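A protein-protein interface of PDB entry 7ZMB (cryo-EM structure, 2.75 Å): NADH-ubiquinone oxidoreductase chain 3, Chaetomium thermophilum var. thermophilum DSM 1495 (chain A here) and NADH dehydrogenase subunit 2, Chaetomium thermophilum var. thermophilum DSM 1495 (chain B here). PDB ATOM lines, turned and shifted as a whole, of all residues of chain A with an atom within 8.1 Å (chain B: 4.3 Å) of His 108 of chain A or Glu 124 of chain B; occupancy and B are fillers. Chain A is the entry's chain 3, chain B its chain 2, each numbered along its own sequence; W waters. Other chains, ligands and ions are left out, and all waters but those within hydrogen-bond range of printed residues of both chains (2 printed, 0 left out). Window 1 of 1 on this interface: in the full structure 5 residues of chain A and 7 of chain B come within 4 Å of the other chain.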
ATOM      1  N   PHE A 102       3.784  13.461 -11.590  1.00  0.00           N
ATOM      2  CA  PHE A 102       2.932  12.301 -11.808  1.00  0.00           C
ATOM      3  C   PHE A 102       2.088  12.469 -13.065  1.00  0.00           C
ATOM      4  O   PHE A 102       1.832  11.498 -13.781  1.00  0.00           O
ATOM      5  CB  PHE A 102       2.047  12.062 -10.583  1.00  0.00           C
ATOM      6  CG  PHE A 102       1.322  10.754 -10.610  1.00  0.00           C
ATOM      7  CD1 PHE A 102       1.969   9.598 -11.003  1.00  0.00           C
ATOM      8  CD2 PHE A 102      -0.006  10.681 -10.264  1.00  0.00           C
ATOM      9  CE1 PHE A 102       1.307   8.400 -11.035  1.00  0.00           C
ATOM     10  CE2 PHE A 102      -0.673   9.475 -10.297  1.00  0.00           C
ATOM     11  CZ  PHE A 102      -0.018   8.340 -10.680  1.00  0.00           C
ATOM     12  N   VAL A 103       1.630  13.686 -13.343  1.00  0.00           N
ATOM     13  CA  VAL A 103       0.860  13.958 -14.594  1.00  0.00           C
ATOM     14  C   VAL A 103       1.820  13.775 -15.772  1.00  0.00           C
ATOM     15  O   VAL A 103       1.368  13.342 -16.846  1.00  0.00           O
ATOM     16  CB  VAL A 103       0.246  15.373 -14.545  1.00  0.00           C
ATOM     17  CG1 VAL A 103      -0.217  15.875 -15.904  1.00  0.00           C
ATOM     18  CG2 VAL A 103      -0.862  15.483 -13.513  1.00  0.00           C
ATOM     19  N   TYR A 104       3.106  14.058 -15.569  1.00  0.00           N
ATOM     20  CA  TYR A 104       4.127  13.811 -16.618  1.00  0.00           C
ATOM     21  C   TYR A 104       4.223  12.311 -16.918  1.00  0.00           C
ATOM     22  O   TYR A 104       4.414  11.946 -18.088  1.00  0.00           O
ATOM     23  CB  TYR A 104       5.479  14.399 -16.210  1.00  0.00           C
ATOM     24  CG  TYR A 104       6.620  13.997 -17.110  1.00  0.00           C
ATOM     25  CD1 TYR A 104       6.888  14.688 -18.281  1.00  0.00           C
ATOM     26  CD2 TYR A 104       7.428  12.916 -16.797  1.00  0.00           C
ATOM     27  CE1 TYR A 104       7.930  14.320 -19.113  1.00  0.00           C
ATOM     28  CE2 TYR A 104       8.469  12.530 -17.623  1.00  0.00           C
ATOM     29  CZ  TYR A 104       8.724  13.237 -18.782  1.00  0.00           C
ATOM     30  OH  TYR A 104       9.757  12.860 -19.589  1.00  0.00           O
ATOM     31  N   GLU A 105       4.065  11.472 -15.899  1.00  0.00           N
ATOM     32  CA  GLU A 105       4.234  10.010 -16.091  1.00  0.00           C
ATOM     33  C   GLU A 105       2.967   9.434 -16.721  1.00  0.00           C
ATOM     34  O   GLU A 105       3.092   8.473 -17.489  1.00  0.00           O
ATOM     35  CB  GLU A 105       4.479   9.294 -14.760  1.00  0.00           C
ATOM     36  CG  GLU A 105       5.573   9.894 -13.904  1.00  0.00           C
ATOM     37  CD  GLU A 105       7.004   9.710 -14.374  1.00  0.00           C
ATOM     38  OE1 GLU A 105       7.900   9.728 -13.515  1.00  0.00           O
ATOM     39  OE2 GLU A 105       7.222   9.561 -15.589  1.00  0.00           O
ATOM     40  N   LEU A 106       1.799  10.010 -16.428  1.00  0.00           N
ATOM     41  CA  LEU A 106       0.577   9.546 -17.070  1.00  0.00           C
ATOM     42  C   LEU A 106       0.470  10.053 -18.500  1.00  0.00           C
ATOM     43  O   LEU A 106       0.064   9.308 -19.399  1.00  0.00           O
ATOM     44  CB  LEU A 106      -0.644   9.973 -16.260  1.00  0.00           C
ATOM     45  CG  LEU A 106      -0.856   9.286 -14.911  1.00  0.00           C
ATOM     46  CD1 LEU A 106      -1.530  10.228 -13.943  1.00  0.00           C
ATOM     47  CD2 LEU A 106      -1.659   8.016 -15.068  1.00  0.00           C
ATOM     48  N   GLY A 107       0.844  11.306 -18.728  1.00  0.00           N
ATOM     49  CA  GLY A 107       0.756  11.955 -20.051  1.00  0.00           C
ATOM     50  C   GLY A 107       1.610  11.294 -21.108  1.00  0.00           C
ATOM     51  O   GLY A 107       1.158  11.204 -22.250  1.00  0.00           O
ATOM     52  N   HIS A 108       2.813  10.859 -20.745  1.00  0.00           N
ATOM     53  CA  HIS A 108       3.767  10.304 -21.741  1.00  0.00           C
ATOM     54  C   HIS A 108       3.553   8.801 -21.937  1.00  0.00           C
ATOM     55  O   HIS A 108       4.202   8.253 -22.842  1.00  0.00           O
ATOM     56  CB  HIS A 108       5.201  10.685 -21.355  1.00  0.00           C
ATOM     57  CG  HIS A 108       5.562  12.085 -21.710  1.00  0.00           C
ATOM     58  ND1 HIS A 108       6.706  12.393 -22.411  1.00  0.00           N
ATOM     59  CD2 HIS A 108       4.923  13.252 -21.493  1.00  0.00           C
ATOM     60  CE1 HIS A 108       6.762  13.693 -22.602  1.00  0.00           C
ATOM     61  NE2 HIS A 108       5.683  14.239 -22.046  1.00  0.00           N
ATOM     62  N   ASP A 109       2.724   8.174 -21.097  1.00  0.00           N
ATOM     63  CA  ASP A 109       2.419   6.720 -21.181  1.00  0.00           C
ATOM     64  C   ASP A 109       3.634   5.970 -20.655  1.00  0.00           C
ATOM     65  O   ASP A 109       3.952   4.893 -21.195  1.00  0.00           O
ATOM     66  CB  ASP A 109       1.939   6.272 -22.565  1.00  0.00           C
ATOM     67  CG  ASP A 109       0.490   6.632 -22.845  1.00  0.00           C
ATOM     68  OD1 ASP A 109      -0.288   6.726 -21.876  1.00  0.00           O
ATOM     69  OD2 ASP A 109       0.151   6.815 -24.031  1.00  0.00           O
ATOM     70  N   ALA A 110       4.318   6.554 -19.680  1.00  0.00           N
ATOM     71  CA  ALA A 110       5.443   5.878 -19.057  1.00  0.00           C
ATOM     72  C   ALA A 110       5.013   4.656 -18.263  1.00  0.00           C
ATOM     73  O   ALA A 110       5.854   3.815 -17.941  1.00  0.00           O
ATOM     74  CB  ALA A 110       6.199   6.840 -18.142  1.00  0.00           C
ATOM     75  N   LEU A 111       3.736   4.600 -17.901  1.00  0.00           N
ATOM     76  CA  LEU A 111       3.212   3.495 -17.072  1.00  0.00           C
ATOM     77  C   LEU A 111       2.342   2.642 -17.981  1.00  0.00           C
ATOM     78  O   LEU A 111       1.206   2.329 -17.594  1.00  0.00           O
ATOM     79  CB  LEU A 111       2.394   4.108 -15.934  1.00  0.00           C
ATOM     80  CG  LEU A 111       3.155   5.090 -15.044  1.00  0.00           C
ATOM     81  CD1 LEU A 111       2.215   5.813 -14.095  1.00  0.00           C
ATOM     82  CD2 LEU A 111       4.259   4.381 -14.276  1.00  0.00           C
ATOM     83  N   LYS A 112       2.870   2.295 -19.157  1.00  0.00           N
ATOM     84  CA  LYS A 112       2.059   1.537 -20.135  1.00  0.00           C
ATOM     85  C   LYS A 112       2.904   0.426 -20.737  1.00  0.00           C
ATOM     86  O   LYS A 112       3.988   0.731 -21.273  1.00  0.00           O
ATOM     87  CB  LYS A 112       1.551   2.460 -21.241  1.00  0.00           C
ATOM     88  CG  LYS A 112       0.472   1.861 -22.134  1.00  0.00           C
ATOM     89  CD  LYS A 112       0.155   2.714 -23.342  1.00  0.00           C
ATOM     90  CE  LYS A 112       1.318   2.813 -24.307  1.00  0.00           C
ATOM     91  NZ  LYS A 112       1.701   1.484 -24.841  1.00  0.00           N
ATOM     92  N   THR B  13       4.639  20.230 -21.484  1.00  0.00           N
ATOM     93  CA  THR B  13       5.468  19.115 -22.007  1.00  0.00           C
ATOM     94  C   THR B  13       4.798  17.780 -21.696  1.00  0.00           C
ATOM     95  O   THR B  13       4.902  16.883 -22.539  1.00  0.00           O
ATOM     96  CB  THR B  13       6.879  19.185 -21.413  1.00  0.00           C
ATOM     97  OG1 THR B  13       7.434  20.439 -21.809  1.00  0.00           O
ATOM     98  CG2 THR B  13       7.787  18.062 -21.864  1.00  0.00           C
ATOM     99  N   SER B  14       4.091  17.667 -20.572  1.00  0.00           N
ATOM    100  CA  SER B  14       3.552  16.363 -20.121  1.00  0.00           C
ATOM    101  C   SER B  14       2.274  15.933 -20.856  1.00  0.00           C
ATOM    102  O   SER B  14       1.858  14.791 -20.659  1.00  0.00           O
ATOM    103  CB  SER B  14       3.308  16.435 -18.647  1.00  0.00           C
ATOM    104  OG  SER B  14       2.237  17.316 -18.353  1.00  0.00           O
ATOM    105  N   THR B  16       2.067  16.251 -24.335  1.00  0.00           N
ATOM    106  CA  THR B  16       2.452  16.142 -25.733  1.00  0.00           C
ATOM    107  C   THR B  16       3.575  15.131 -25.868  1.00  0.00           C
ATOM    108  O   THR B  16       4.454  15.047 -25.008  1.00  0.00           O
ATOM    109  CB  THR B  16       2.891  17.508 -26.317  1.00  0.00           C
ATOM    110  OG1 THR B  16       3.243  17.369 -27.699  1.00  0.00           O
ATOM    111  CG2 THR B  16       4.071  18.088 -25.559  1.00  0.00           C
ATOM    112  N   LEU B  17       3.523  14.340 -26.934  1.00  0.00           N
ATOM    113  CA  LEU B  17       4.682  13.586 -27.395  1.00  0.00           C
ATOM    114  C   LEU B  17       5.116  14.030 -28.787  1.00  0.00           C
ATOM    115  O   LEU B  17       5.817  13.290 -29.481  1.00  0.00           O
ATOM    116  CB  LEU B  17       4.418  12.079 -27.367  1.00  0.00           C
ATOM    117  CG  LEU B  17       4.603  11.316 -26.049  1.00  0.00           C
ATOM    118  CD1 LEU B  17       6.064  11.366 -25.602  1.00  0.00           C
ATOM    119  CD2 LEU B  17       3.691  11.798 -24.943  1.00  0.00           C
ATOM    120  N   ILE B 122      14.534  16.771 -29.020  1.00  0.00           N
ATOM    121  CA  ILE B 122      14.382  16.428 -27.571  1.00  0.00           C
ATOM    122  C   ILE B 122      13.490  17.465 -26.889  1.00  0.00           C
ATOM    123  O   ILE B 122      13.982  18.567 -26.630  1.00  0.00           O
ATOM    124  CB  ILE B 122      15.750  16.240 -26.887  1.00  0.00           C
ATOM    125  CG1 ILE B 122      16.618  15.244 -27.661  1.00  0.00           C
ATOM    126  CG2 ILE B 122      15.573  15.828 -25.437  1.00  0.00           C
ATOM    127  CD1 ILE B 122      18.037  15.161 -27.173  1.00  0.00           C
ATOM    128  N   ILE B 123      12.177  16.890 -26.577  1.00  0.00           N
ATOM    129  CA  ILE B 123      11.117  17.765 -25.991  1.00  0.00           C
ATOM    130  C   ILE B 123      11.533  18.311 -24.619  1.00  0.00           C
ATOM    131  O   ILE B 123      11.372  19.523 -24.415  1.00  0.00           O
ATOM    132  CB  ILE B 123       9.773  17.010 -25.947  1.00  0.00           C
ATOM    133  CG1 ILE B 123       9.606  16.099 -27.167  1.00  0.00           C
ATOM    134  CG2 ILE B 123       8.608  17.973 -25.801  1.00  0.00           C
ATOM    135  CD1 ILE B 123       8.319  15.313 -27.179  1.00  0.00           C
ATOM    136  N   GLU B 124      12.151  17.596 -23.786  1.00  0.00           N
ATOM    137  CA  GLU B 124      12.433  17.904 -22.360  1.00  0.00           C
ATOM    138  C   GLU B 124      13.770  18.636 -22.195  1.00  0.00           C
ATOM    139  O   GLU B 124      14.075  19.019 -21.067  1.00  0.00           O
ATOM    140  CB  GLU B 124      12.385  16.619 -21.523  1.00  0.00           C
ATOM    141  CG  GLU B 124      11.081  15.846 -21.629  1.00  0.00           C
ATOM    142  CD  GLU B 124      10.923  14.899 -22.812  1.00  0.00           C
ATOM    143  OE1 GLU B 124       9.944  14.135 -22.817  1.00  0.00           O
ATOM    144  OE2 GLU B 124      11.774  14.922 -23.722  1.00  0.00           O
ATOM    145  N   TYR B 125      14.543  18.814 -23.263  1.00  0.00           N
ATOM    146  CA  TYR B 125      15.899  19.420 -23.145  1.00  0.00           C
ATOM    147  C   TYR B 125      15.864  20.801 -22.456  1.00  0.00           C
ATOM    148  O   TYR B 125      16.631  20.932 -21.488  1.00  0.00           O
ATOM    149  CB  TYR B 125      16.598  19.416 -24.505  1.00  0.00           C
ATOM    150  CG  TYR B 125      18.042  19.844 -24.489  1.00  0.00           C
ATOM    151  CD1 TYR B 125      19.049  18.923 -24.264  1.00  0.00           C
ATOM    152  CD2 TYR B 125      18.404  21.162 -24.715  1.00  0.00           C
ATOM    153  CE1 TYR B 125      20.381  19.300 -24.253  1.00  0.00           C
ATOM    154  CE2 TYR B 125      19.731  21.557 -24.703  1.00  0.00           C
ATOM    155  CZ  TYR B 125      20.721  20.621 -24.472  1.00  0.00           C
ATOM    156  OH  TYR B 125      22.032  20.992 -24.458  1.00  0.00           O
ATOM    157  N   PRO B 126      15.085  21.834 -22.880  1.00  0.00           N
ATOM    158  CA  PRO B 126      15.077  23.115 -22.171  1.00  0.00           C
ATOM    159  C   PRO B 126      14.667  22.924 -20.703  1.00  0.00           C
ATOM    160  O   PRO B 126      15.216  23.590 -19.864  1.00  0.00           O
ATOM    161  CB  PRO B 126      14.053  23.975 -22.931  1.00  0.00           C
ATOM    162  CG  PRO B 126      13.175  22.979 -23.634  1.00  0.00           C
ATOM    163  CD  PRO B 126      14.136  21.877 -24.015  1.00  0.00           C
ATOM    164  N   LEU B 127      13.759  21.989 -20.440  1.00  0.00           N
ATOM    165  CA  LEU B 127      13.251  21.756 -19.070  1.00  0.00           C
ATOM    166  C   LEU B 127      14.371  21.301 -18.134  1.00  0.00           C
ATOM    167  O   LEU B 127      14.443  21.841 -17.030  1.00  0.00           O
ATOM    168  CB  LEU B 127      12.196  20.660 -19.205  1.00  0.00           C
ATOM    169  CG  LEU B 127      11.141  20.595 -18.108  1.00  0.00           C
ATOM    170  CD1 LEU B 127       9.760  20.600 -18.731  1.00  0.00           C
ATOM    171  CD2 LEU B 127      11.335  19.348 -17.263  1.00  0.00           C
ATOM    172  N   ILE B 128      15.178  20.322 -18.556  1.00  0.00           N
ATOM    173  CA  ILE B 128      16.313  19.812 -17.732  1.00  0.00           C
ATOM    174  C   ILE B 128      17.341  20.932 -17.560  1.00  0.00           C
ATOM    175  O   ILE B 128      17.906  21.043 -16.468  1.00  0.00           O
ATOM    176  CB  ILE B 128      16.911  18.533 -18.354  1.00  0.00           C
ATOM    177  CG1 ILE B 128      15.817  17.498 -18.632  1.00  0.00           C
ATOM    178  CG2 ILE B 128      18.020  17.961 -17.486  1.00  0.00           C
ATOM    179  CD1 ILE B 128      16.311  16.075 -18.678  1.00  0.00           C
HETATM  180  O   HOH W   1       9.927  11.505 -21.937  1.00  0.00           O
HETATM  181  O   HOH W   2       0.819  13.097 -24.735  1.00  0.00           O
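The backbone carbonyl oxygen of Thr 13 of chain B sits at hydrogen-bond distance from a ring nitrogen (NE2) of His 108 of chain A, at 2.8 Å. O of Thr 16 of chain B sits at hydrogen-bond distance from NE2 of His 108 of chain A (3.3 Å). The side-chain carboxylate of Glu 124 of chain B lies within hydrogen-bond range of the side-chain hydroxyl of Tyr 104 of chain A, 3.5 Å away.
CG1 of Val 103 of chain A touches OG of Ser 14 of chain B, at 3.8 Å. Ser 14 of chain B touches Tyr 104 of chain A (CB to CA, 3.4 Å). Gly 107 of chain A touches Ser 14 of chain B. CD2 of Leu 17 of chain B touches O of Gly 107 of chain A (3.7 Å). His 108 of chain A touches Ser 14 of chain B. Leu 17 of chain B touches His 108 of chain A (CD1 to ND1, 3.4 Å). CE1 of His 108 of chain A touches OE1 of Glu 124 of chain B, at 3.2 Å.
Of the printed residues of chain B, Tyr 104 of chain A touches Ser 14 (3.4 Å) and Glu 124 (3.5 Å). Of the printed residues of chain B, Gly 107 of chain A touches Ser 14 (3.1 Å) and Leu 17 (3.7 Å). His 108 of chain A touches just these residues of chain B: Thr 13 (2.8 Å), Ser 14 (3.5 Å), Thr 16 (3.3 Å), Leu 17 (3.4 Å) and Glu 124 (3.2 Å). Printed residues of chain A within 4 Å of Thr 13 of chain B: His 108 (2.8 Å). Of the printed residues of chain A, Ser 14 of chain B touches Val 103, Tyr 104, Gly 107 and His 108. Of the printed residues of chain A, Leu 17 of chain B touches Gly 107 (3.7 Å) and His 108 (3.4 Å). Of chain A, only Tyr 104 and His 108 come within 4 Å of Glu 124 of chain B. The nearest printed residue of chain B that does not touch His 108 of chain A is Ile 123 of chain B (5.1 Å). The nearest printed residue of chain A that does not touch Glu 124 of chain B is Gly 107 of chain A (9.0 Å). The nearest printed residue of chain A that does not touch Thr 13 of chain B is Tyr 104 of chain A (4.6 Å).
Of the 11 printed residues of chain B, 5 touch a printed residue of chain A. Hydrophobic or aromatic side chains of chain B that line the printed part of chain A: Leu 17. Hydrophobic or aromatic side chains of chain A that line the printed part of chain B: Val 103, Tyr 104 and His 108. Among the printed residues, no Asp or Glu carboxylate lies within 4 Å of a Lys or Arg side-chain nitrogen of the other chain.
Water W1 lies within hydrogen-bond range of OH of Tyr 104 of chain A, OE1 of Glu 124 of chain B and ND1 of His 108 of chain A. Water W2 lies within hydrogen-bond range of O of Gly 107 of chain A (3.1 Å) and N of Thr 16 of chain B (3.4 Å).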
